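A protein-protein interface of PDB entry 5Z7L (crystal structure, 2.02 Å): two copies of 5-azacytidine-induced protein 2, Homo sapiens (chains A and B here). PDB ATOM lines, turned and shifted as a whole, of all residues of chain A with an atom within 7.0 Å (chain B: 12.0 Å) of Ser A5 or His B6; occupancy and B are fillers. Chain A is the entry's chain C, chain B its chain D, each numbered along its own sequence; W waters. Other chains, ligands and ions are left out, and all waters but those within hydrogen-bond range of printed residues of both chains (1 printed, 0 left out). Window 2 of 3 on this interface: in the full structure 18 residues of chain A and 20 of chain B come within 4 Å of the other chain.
Among the printed residues, pairs that only touch across the chains: Leu A9 with His B6, Leu A9 with Leu B9, Leu A9 with Val B10 and Val A10 with Leu B9.
A ring nitrogen (NE2) of His B6 lies within hydrogen-bond range of the side-chain hydroxyl (OG) of Ser A5 (3.2 Å).
A ring nitrogen (NE2) of His A6 sits at hydrogen-bond distance from the side-chain hydroxyl (OG) of Ser B5 (3.3 Å).
Water W1 bridges O of Ser A5 (2.7 Å) and NE2 of His B6 (3.2 Å).
Of the 10 printed residues of chain A, 4 touch a printed residue of chain B.
Printed residues of chain A that touch a printed residue of chain B: Ser A5, His A6, Leu A9 and Val A10.
Hydrophobic or aromatic side chains of chain A that line the printed part of chain B: His A6, Leu A9 and Val A10.
Along chain A the printed residues that touch a printed residue of chain B span positions 5 to 10.
Of the 17 printed residues of chain B, 4 touch a printed residue of chain A.
Printed residues of chain B that touch a printed residue of chain A: Ser B5, His B6, Leu B9 and Val B10.
Hydrophobic or aromatic side chains of chain B that line the printed part of chain A: His B6, Leu B9 and Val B10.
Among the printed residues, 6 pairs touch across the chains.
Among the printed residues, no Asp or Glu carboxylate lies within 4 Å of a Lys or Arg side-chain nitrogen of the other chain.
Ser A5 touches His B6, and with the chains exchanged His A6 touches Ser B5.
Leu A9 touches His B6, but with the chains exchanged His A6 does not touch Leu B9 (4.04 Å).
Leu A9 touches its own counterpart, Leu B9.
Leu A9 touches Val B10, and with the chains exchanged Val A10 touches Leu B9.
Positions printed for both chains: 1, 2, 3, 4, 5, 6, 7, 8, 9 and 10.
Of the 6 pairs that touch across the chains among the printed residues, 5 have their exchanged pair printed and touching as well.
No residue of chain B comes within 4 Å of Val A3.
Of chain B, only Ser B5 (3.3 Å) comes within 4 Å of His A6.
No residue of chain B comes within 4 Å of Ala A8.
Of chain B, only His B6 (3.6 Å), Leu B9 (3.5 Å) and Val B10 (3.5 Å) come within 4 Å of Leu A9.
Of the printed residues of chain B, Val A10 touches Leu B9 (3.6 Å).
Printed residues of chain A within 4 Å of Ser B5: His A6 (3.3 Å).
Of chain A, only Ser A5 (3.2 Å) and Leu A9 (3.6 Å) come within 4 Å of His B6.
Of the printed residues of chain A, Leu B9 touches Leu A9 and Val A10.
Printed residues of chain A within 4 Å of Val B10: Leu A9 (3.5 Å).
The nearest residue of chain B that does not touch Ser A5 is Leu B9 (6.5 Å).
The nearest residue of chain A that does not touch His B6 is His A6 (4.2 Å).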
ATOM      1  N   GLU A   1      28.726  23.447   7.386  1.00  0.00           N
ATOM      2  CA  GLU A   1      28.933  24.360   6.261  1.00  0.00           C
ATOM      3  C   GLU A   1      27.621  24.604   5.546  1.00  0.00           C
ATOM      4  O   GLU A   1      27.131  25.735   5.490  1.00  0.00           O
ATOM      5  CB  GLU A   1      29.960  23.804   5.273  1.00  0.00           C
ATOM      6  CG  GLU A   1      30.273  24.744   4.119  1.00  0.00           C
ATOM      7  CD  GLU A   1      31.518  25.578   4.370  1.00  0.00           C
ATOM      8  OE1 GLU A   1      31.520  26.794   4.048  1.00  0.00           O
ATOM      9  OE2 GLU A   1      32.499  25.010   4.895  1.00  0.00           O
ATOM     10  N   SER A   2      27.065  23.533   4.976  1.00  0.00           N
ATOM     11  CA  SER A   2      25.706  23.598   4.454  1.00  0.00           C
ATOM     12  C   SER A   2      24.702  23.889   5.556  1.00  0.00           C
ATOM     13  O   SER A   2      23.603  24.366   5.261  1.00  0.00           O
ATOM     14  CB  SER A   2      25.339  22.294   3.735  1.00  0.00           C
ATOM     15  OG  SER A   2      24.782  21.346   4.637  1.00  0.00           O
ATOM     16  N   VAL A   3      25.050  23.604   6.816  1.00  0.00           N
ATOM     17  CA  VAL A   3      24.164  23.928   7.929  1.00  0.00           C
ATOM     18  C   VAL A   3      24.216  25.415   8.240  1.00  0.00           C
ATOM     19  O   VAL A   3      23.176  26.079   8.361  1.00  0.00           O
ATOM     20  CB  VAL A   3      24.516  23.081   9.167  1.00  0.00           C
ATOM     21  CG1 VAL A   3      23.457  23.275  10.255  1.00  0.00           C
ATOM     22  CG2 VAL A   3      24.625  21.610   8.782  1.00  0.00           C
ATOM     23  N   ALA A   4      25.424  25.964   8.394  1.00  0.00           N
ATOM     24  CA  ALA A   4      25.542  27.413   8.521  1.00  0.00           C
ATOM     25  C   ALA A   4      24.957  28.107   7.297  1.00  0.00           C
ATOM     26  O   ALA A   4      24.260  29.117   7.428  1.00  0.00           O
ATOM     27  CB  ALA A   4      27.005  27.808   8.735  1.00  0.00           C
ATOM     28  N   SER A   5      25.201  27.557   6.102  1.00  0.00           N
ATOM     29  CA  SER A   5      24.662  28.155   4.882  1.00  0.00           C
ATOM     30  C   SER A   5      23.147  28.251   4.943  1.00  0.00           C
ATOM     31  O   SER A   5      22.557  29.286   4.606  1.00  0.00           O
ATOM     32  CB  SER A   5      25.081  27.340   3.659  1.00  0.00           C
ATOM     33  OG  SER A   5      24.354  27.769   2.517  1.00  0.00           O
ATOM     34  N   HIS A   6      22.497  27.165   5.358  1.00  0.00           N
ATOM     35  CA  HIS A   6      21.046  27.151   5.434  1.00  0.00           C
ATOM     36  C   HIS A   6      20.562  28.095   6.519  1.00  0.00           C
ATOM     37  O   HIS A   6      19.629  28.881   6.308  1.00  0.00           O
ATOM     38  CB  HIS A   6      20.570  25.729   5.698  1.00  0.00           C
ATOM     39  CG  HIS A   6      19.087  25.595   5.733  1.00  0.00           C
ATOM     40  ND1 HIS A   6      18.341  25.921   6.845  1.00  0.00           N
ATOM     41  CD2 HIS A   6      18.211  25.158   4.799  1.00  0.00           C
ATOM     42  CE1 HIS A   6      17.064  25.688   6.592  1.00  0.00           C
ATOM     43  NE2 HIS A   6      16.960  25.225   5.359  1.00  0.00           N
ATOM     44  N   PHE A   7      21.192  28.031   7.694  1.00  0.00           N
ATOM     45  CA  PHE A   7      20.848  28.950   8.774  1.00  0.00           C
ATOM     46  C   PHE A   7      20.942  30.408   8.327  1.00  0.00           C
ATOM     47  O   PHE A   7      20.060  31.221   8.636  1.00  0.00           O
ATOM     48  CB  PHE A   7      21.766  28.702   9.970  1.00  0.00           C
ATOM     49  CG  PHE A   7      21.511  29.624  11.122  1.00  0.00           C
ATOM     50  CD1 PHE A   7      20.487  29.365  12.019  1.00  0.00           C
ATOM     51  CD2 PHE A   7      22.284  30.758  11.305  1.00  0.00           C
ATOM     52  CE1 PHE A   7      20.244  30.219  13.079  1.00  0.00           C
ATOM     53  CE2 PHE A   7      22.042  31.611  12.362  1.00  0.00           C
ATOM     54  CZ  PHE A   7      21.024  31.339  13.251  1.00  0.00           C
ATOM     55  N   ALA A   8      22.014  30.765   7.613  1.00  0.00           N
ATOM     56  CA  ALA A   8      22.180  32.156   7.220  1.00  0.00           C
ATOM     57  C   ALA A   8      21.087  32.583   6.263  1.00  0.00           C
ATOM     58  O   ALA A   8      20.654  33.738   6.298  1.00  0.00           O
ATOM     59  CB  ALA A   8      23.550  32.376   6.579  1.00  0.00           C
ATOM     60  N   LEU A   9      20.623  31.659   5.413  1.00  0.00           N
ATOM     61  CA  LEU A   9      19.560  31.984   4.476  1.00  0.00           C
ATOM     62  C   LEU A   9      18.219  32.096   5.191  1.00  0.00           C
ATOM     63  O   LEU A   9      17.393  32.947   4.838  1.00  0.00           O
ATOM     64  CB  LEU A   9      19.512  30.922   3.371  1.00  0.00           C
ATOM     65  CG  LEU A   9      18.452  31.070   2.268  1.00  0.00           C
ATOM     66  CD1 LEU A   9      18.541  32.432   1.580  1.00  0.00           C
ATOM     67  CD2 LEU A   9      18.586  29.937   1.249  1.00  0.00           C
ATOM     68  N   VAL A  10      17.974  31.223   6.175  1.00  0.00           N
ATOM     69  CA  VAL A  10      16.779  31.334   7.012  1.00  0.00           C
ATOM     70  C   VAL A  10      16.744  32.703   7.675  1.00  0.00           C
ATOM     71  O   VAL A  10      15.722  33.400   7.660  1.00  0.00           O
ATOM     72  CB  VAL A  10      16.744  30.200   8.060  1.00  0.00           C
ATOM     73  CG1 VAL A  10      15.712  30.486   9.162  1.00  0.00           C
ATOM     74  CG2 VAL A  10      16.457  28.861   7.407  1.00  0.00           C
ATOM     75  N   GLU B   1      23.685  16.074   3.824  1.00  0.00           N
ATOM     76  CA  GLU B   1      24.641  16.883   3.077  1.00  0.00           C
ATOM     77  C   GLU B   1      23.977  17.433   1.806  1.00  0.00           C
ATOM     78  O   GLU B   1      24.509  18.331   1.157  1.00  0.00           O
ATOM     79  CB  GLU B   1      25.890  16.054   2.746  1.00  0.00           C
ATOM     80  CG  GLU B   1      26.900  16.741   1.850  1.00  0.00           C
ATOM     81  CD  GLU B   1      27.766  15.760   1.083  1.00  0.00           C
ATOM     82  OE1 GLU B   1      27.886  14.590   1.523  1.00  0.00           O
ATOM     83  OE2 GLU B   1      28.316  16.161   0.036  1.00  0.00           O
ATOM     84  N   SER B   2      22.797  16.903   1.475  1.00  0.00           N
ATOM     85  CA  SER B   2      22.060  17.363   0.302  1.00  0.00           C
ATOM     86  C   SER B   2      21.738  18.849   0.386  1.00  0.00           C
ATOM     87  O   SER B   2      21.396  19.380   1.450  1.00  0.00           O
ATOM     88  CB  SER B   2      20.759  16.584   0.131  1.00  0.00           C
ATOM     89  OG  SER B   2      20.092  16.982  -1.061  1.00  0.00           O
ATOM     90  N   VAL B   3      21.830  19.518  -0.761  1.00  0.00           N
ATOM     91  CA  VAL B   3      21.523  20.934  -0.846  1.00  0.00           C
ATOM     92  C   VAL B   3      20.111  21.191  -1.375  1.00  0.00           C
ATOM     93  O   VAL B   3      19.769  22.332  -1.670  1.00  0.00           O
ATOM     94  CB  VAL B   3      22.578  21.663  -1.691  1.00  0.00           C
ATOM     95  CG1 VAL B   3      23.884  21.756  -0.907  1.00  0.00           C
ATOM     96  CG2 VAL B   3      22.789  20.940  -3.009  1.00  0.00           C
ATOM     97  N   ALA B   4      19.276  20.155  -1.494  1.00  0.00           N
ATOM     98  CA  ALA B   4      17.919  20.376  -1.996  1.00  0.00           C
ATOM     99  C   ALA B   4      17.150  21.352  -1.111  1.00  0.00           C
ATOM    100  O   ALA B   4      16.443  22.232  -1.609  1.00  0.00           O
ATOM    101  CB  ALA B   4      17.181  19.036  -2.085  1.00  0.00           C
ATOM    102  N   SER B   5      17.283  21.213   0.209  1.00  0.00           N
ATOM    103  CA  SER B   5      16.575  22.082   1.142  1.00  0.00           C
ATOM    104  C   SER B   5      16.986  23.540   0.970  1.00  0.00           C
ATOM    105  O   SER B   5      16.159  24.453   1.077  1.00  0.00           O
ATOM    106  CB  SER B   5      16.858  21.612   2.568  1.00  0.00           C
ATOM    107  OG  SER B   5      16.439  22.545   3.528  1.00  0.00           O
ATOM    108  N   HIS B   6      18.271  23.774   0.740  1.00  0.00           N
ATOM    109  CA  HIS B   6      18.732  25.128   0.483  1.00  0.00           C
ATOM    110  C   HIS B   6      18.137  25.655  -0.813  1.00  0.00           C
ATOM    111  O   HIS B   6      17.671  26.796  -0.872  1.00  0.00           O
ATOM    112  CB  HIS B   6      20.260  25.132   0.434  1.00  0.00           C
ATOM    113  CG  HIS B   6      20.864  26.494   0.343  1.00  0.00           C
ATOM    114  ND1 HIS B   6      20.999  27.167  -0.851  1.00  0.00           N
ATOM    115  CD2 HIS B   6      21.398  27.296   1.294  1.00  0.00           C
ATOM    116  CE1 HIS B   6      21.593  28.328  -0.631  1.00  0.00           C
ATOM    117  NE2 HIS B   6      21.845  28.430   0.661  1.00  0.00           N
ATOM    118  N   PHE B   7      18.106  24.816  -1.852  1.00  0.00           N
ATOM    119  CA  PHE B   7      17.503  25.234  -3.110  1.00  0.00           C
ATOM    120  C   PHE B   7      16.038  25.612  -2.921  1.00  0.00           C
ATOM    121  O   PHE B   7      15.561  26.603  -3.491  1.00  0.00           O
ATOM    122  CB  PHE B   7      17.641  24.120  -4.139  1.00  0.00           C
ATOM    123  CG  PHE B   7      17.025  24.451  -5.465  1.00  0.00           C
ATOM    124  CD1 PHE B   7      17.737  25.166  -6.412  1.00  0.00           C
ATOM    125  CD2 PHE B   7      15.732  24.042  -5.765  1.00  0.00           C
ATOM    126  CE1 PHE B   7      17.168  25.483  -7.636  1.00  0.00           C
ATOM    127  CE2 PHE B   7      15.164  24.352  -6.977  1.00  0.00           C
ATOM    128  CZ  PHE B   7      15.880  25.076  -7.916  1.00  0.00           C
ATOM    129  N   ALA B   8      15.306  24.820  -2.133  1.00  0.00           N
ATOM    130  CA  ALA B   8      13.893  25.099  -1.902  1.00  0.00           C
ATOM    131  C   ALA B   8      13.704  26.449  -1.234  1.00  0.00           C
ATOM    132  O   ALA B   8      12.758  27.182  -1.541  1.00  0.00           O
ATOM    133  CB  ALA B   8      13.271  24.004  -1.041  1.00  0.00           C
ATOM    134  N   LEU B   9      14.591  26.783  -0.299  1.00  0.00           N
ATOM    135  CA  LEU B   9      14.458  28.038   0.411  1.00  0.00           C
ATOM    136  C   LEU B   9      14.859  29.209  -0.479  1.00  0.00           C
ATOM    137  O   LEU B   9      14.284  30.301  -0.364  1.00  0.00           O
ATOM    138  CB  LEU B   9      15.301  27.994   1.682  1.00  0.00           C
ATOM    139  CG  LEU B   9      15.363  29.230   2.583  1.00  0.00           C
ATOM    140  CD1 LEU B   9      13.989  29.770   2.983  1.00  0.00           C
ATOM    141  CD2 LEU B   9      16.160  28.869   3.814  1.00  0.00           C
ATOM    142  N   VAL B  10      15.838  29.007  -1.369  1.00  0.00           N
ATOM    143  CA  VAL B  10      16.173  30.063  -2.320  1.00  0.00           C
ATOM    144  C   VAL B  10      14.974  30.360  -3.200  1.00  0.00           C
ATOM    145  O   VAL B  10      14.608  31.524  -3.410  1.00  0.00           O
ATOM    146  CB  VAL B  10      17.406  29.685  -3.158  1.00  0.00           C
ATOM    147  CG1 VAL B  10      17.591  30.680  -4.305  1.00  0.00           C
ATOM    148  CG2 VAL B  10      18.657  29.656  -2.280  1.00  0.00           C
ATOM    149  N   THR B  11      14.336  29.307  -3.720  1.00  0.00           N
ATOM    150  CA  THR B  11      13.129  29.493  -4.518  1.00  0.00           C
ATOM    151  C   THR B  11      12.110  30.356  -3.781  1.00  0.00           C
ATOM    152  O   THR B  11      11.492  31.241  -4.381  1.00  0.00           O
ATOM    153  CB  THR B  11      12.512  28.137  -4.868  1.00  0.00           C
ATOM    154  OG1 THR B  11      13.475  27.343  -5.569  1.00  0.00           O
ATOM    155  CG2 THR B  11      11.249  28.302  -5.736  1.00  0.00           C
ATOM    156  N   ALA B  12      11.937  30.122  -2.476  1.00  0.00           N
ATOM    157  CA  ALA B  12      10.937  30.860  -1.701  1.00  0.00           C
ATOM    158  C   ALA B  12      11.395  32.283  -1.428  1.00  0.00           C
ATOM    159  O   ALA B  12      10.628  33.236  -1.598  1.00  0.00           O
ATOM    160  CB  ALA B  12      10.647  30.145  -0.378  1.00  0.00           C
ATOM    161  N   TYR B  13      12.642  32.429  -0.992  1.00  0.00           N
ATOM    162  CA  TYR B  13      13.221  33.743  -0.763  1.00  0.00           C
ATOM    163  C   TYR B  13      13.179  34.600  -2.027  1.00  0.00           C
ATOM    164  O   TYR B  13      12.863  35.796  -1.962  1.00  0.00           O
ATOM    165  CB  TYR B  13      14.656  33.569  -0.248  1.00  0.00           C
ATOM    166  CG  TYR B  13      15.652  34.595  -0.722  1.00  0.00           C
ATOM    167  CD1 TYR B  13      15.680  35.870  -0.181  1.00  0.00           C
ATOM    168  CD2 TYR B  13      16.593  34.275  -1.689  1.00  0.00           C
ATOM    169  CE1 TYR B  13      16.603  36.820  -0.621  1.00  0.00           C
ATOM    170  CE2 TYR B  13      17.519  35.206  -2.127  1.00  0.00           C
ATOM    171  CZ  TYR B  13      17.521  36.472  -1.590  1.00  0.00           C
ATOM    172  OH  TYR B  13      18.452  37.387  -2.035  1.00  0.00           O
ATOM    173  N   GLU B  14      13.495  34.007  -3.185  1.00  0.00           N
ATOM    174  CA  GLU B  14      13.468  34.769  -4.433  1.00  0.00           C
ATOM    175  C   GLU B  14      12.087  35.348  -4.688  1.00  0.00           C
ATOM    176  O   GLU B  14      11.960  36.494  -5.127  1.00  0.00           O
ATOM    177  CB  GLU B  14      13.889  33.889  -5.613  1.00  0.00           C
ATOM    178  CG  GLU B  14      15.384  33.673  -5.769  1.00  0.00           C
ATOM    179  CD  GLU B  14      16.115  34.979  -5.978  1.00  0.00           C
ATOM    180  OE1 GLU B  14      17.218  35.143  -5.417  1.00  0.00           O
ATOM    181  OE2 GLU B  14      15.577  35.844  -6.710  1.00  0.00           O
ATOM    182  N   ASP B  15      11.033  34.576  -4.413  1.00  0.00           N
ATOM    183  CA  ASP B  15       9.696  35.076  -4.704  1.00  0.00           C
ATOM    184  C   ASP B  15       9.227  36.087  -3.669  1.00  0.00           C
ATOM    185  O   ASP B  15       8.513  37.039  -4.007  1.00  0.00           O
ATOM    186  CB  ASP B  15       8.691  33.931  -4.790  1.00  0.00           C
ATOM    187  CG  ASP B  15       7.485  34.301  -5.623  1.00  0.00           C
ATOM    188  OD1 ASP B  15       7.651  34.474  -6.857  1.00  0.00           O
ATOM    189  OD2 ASP B  15       6.386  34.419  -5.046  1.00  0.00           O
ATOM    190  N   ILE B  16       9.584  35.887  -2.402  1.00  0.00           N
ATOM    191  CA  ILE B  16       9.160  36.839  -1.379  1.00  0.00           C
ATOM    192  C   ILE B  16       9.863  38.184  -1.572  1.00  0.00           C
ATOM    193  O   ILE B  16       9.248  39.249  -1.441  1.00  0.00           O
ATOM    194  CB  ILE B  16       9.389  36.228   0.016  1.00  0.00           C
ATOM    195  CG1 ILE B  16       8.310  35.171   0.270  1.00  0.00           C
ATOM    196  CG2 ILE B  16       9.316  37.284   1.102  1.00  0.00           C
ATOM    197  CD1 ILE B  16       8.618  34.246   1.418  1.00  0.00           C
ATOM    198  N   LYS B  17      11.145  38.165  -1.935  1.00  0.00           N
ATOM    199  CA  LYS B  17      11.806  39.433  -2.215  1.00  0.00           C
ATOM    200  C   LYS B  17      11.201  40.125  -3.436  1.00  0.00           C
ATOM    201  O   LYS B  17      11.129  41.356  -3.460  1.00  0.00           O
ATOM    202  CB  LYS B  17      13.317  39.219  -2.352  1.00  0.00           C
ATOM    203  CG  LYS B  17      13.866  39.141  -3.744  1.00  0.00           C
ATOM    204  CD  LYS B  17      15.376  38.800  -3.697  1.00  0.00           C
ATOM    205  CE  LYS B  17      15.913  38.624  -5.106  1.00  0.00           C
ATOM    206  NZ  LYS B  17      17.365  38.299  -5.109  1.00  0.00           N
HETATM  207  O   HOH W   1      22.992  30.856   2.408  1.00  0.00           O
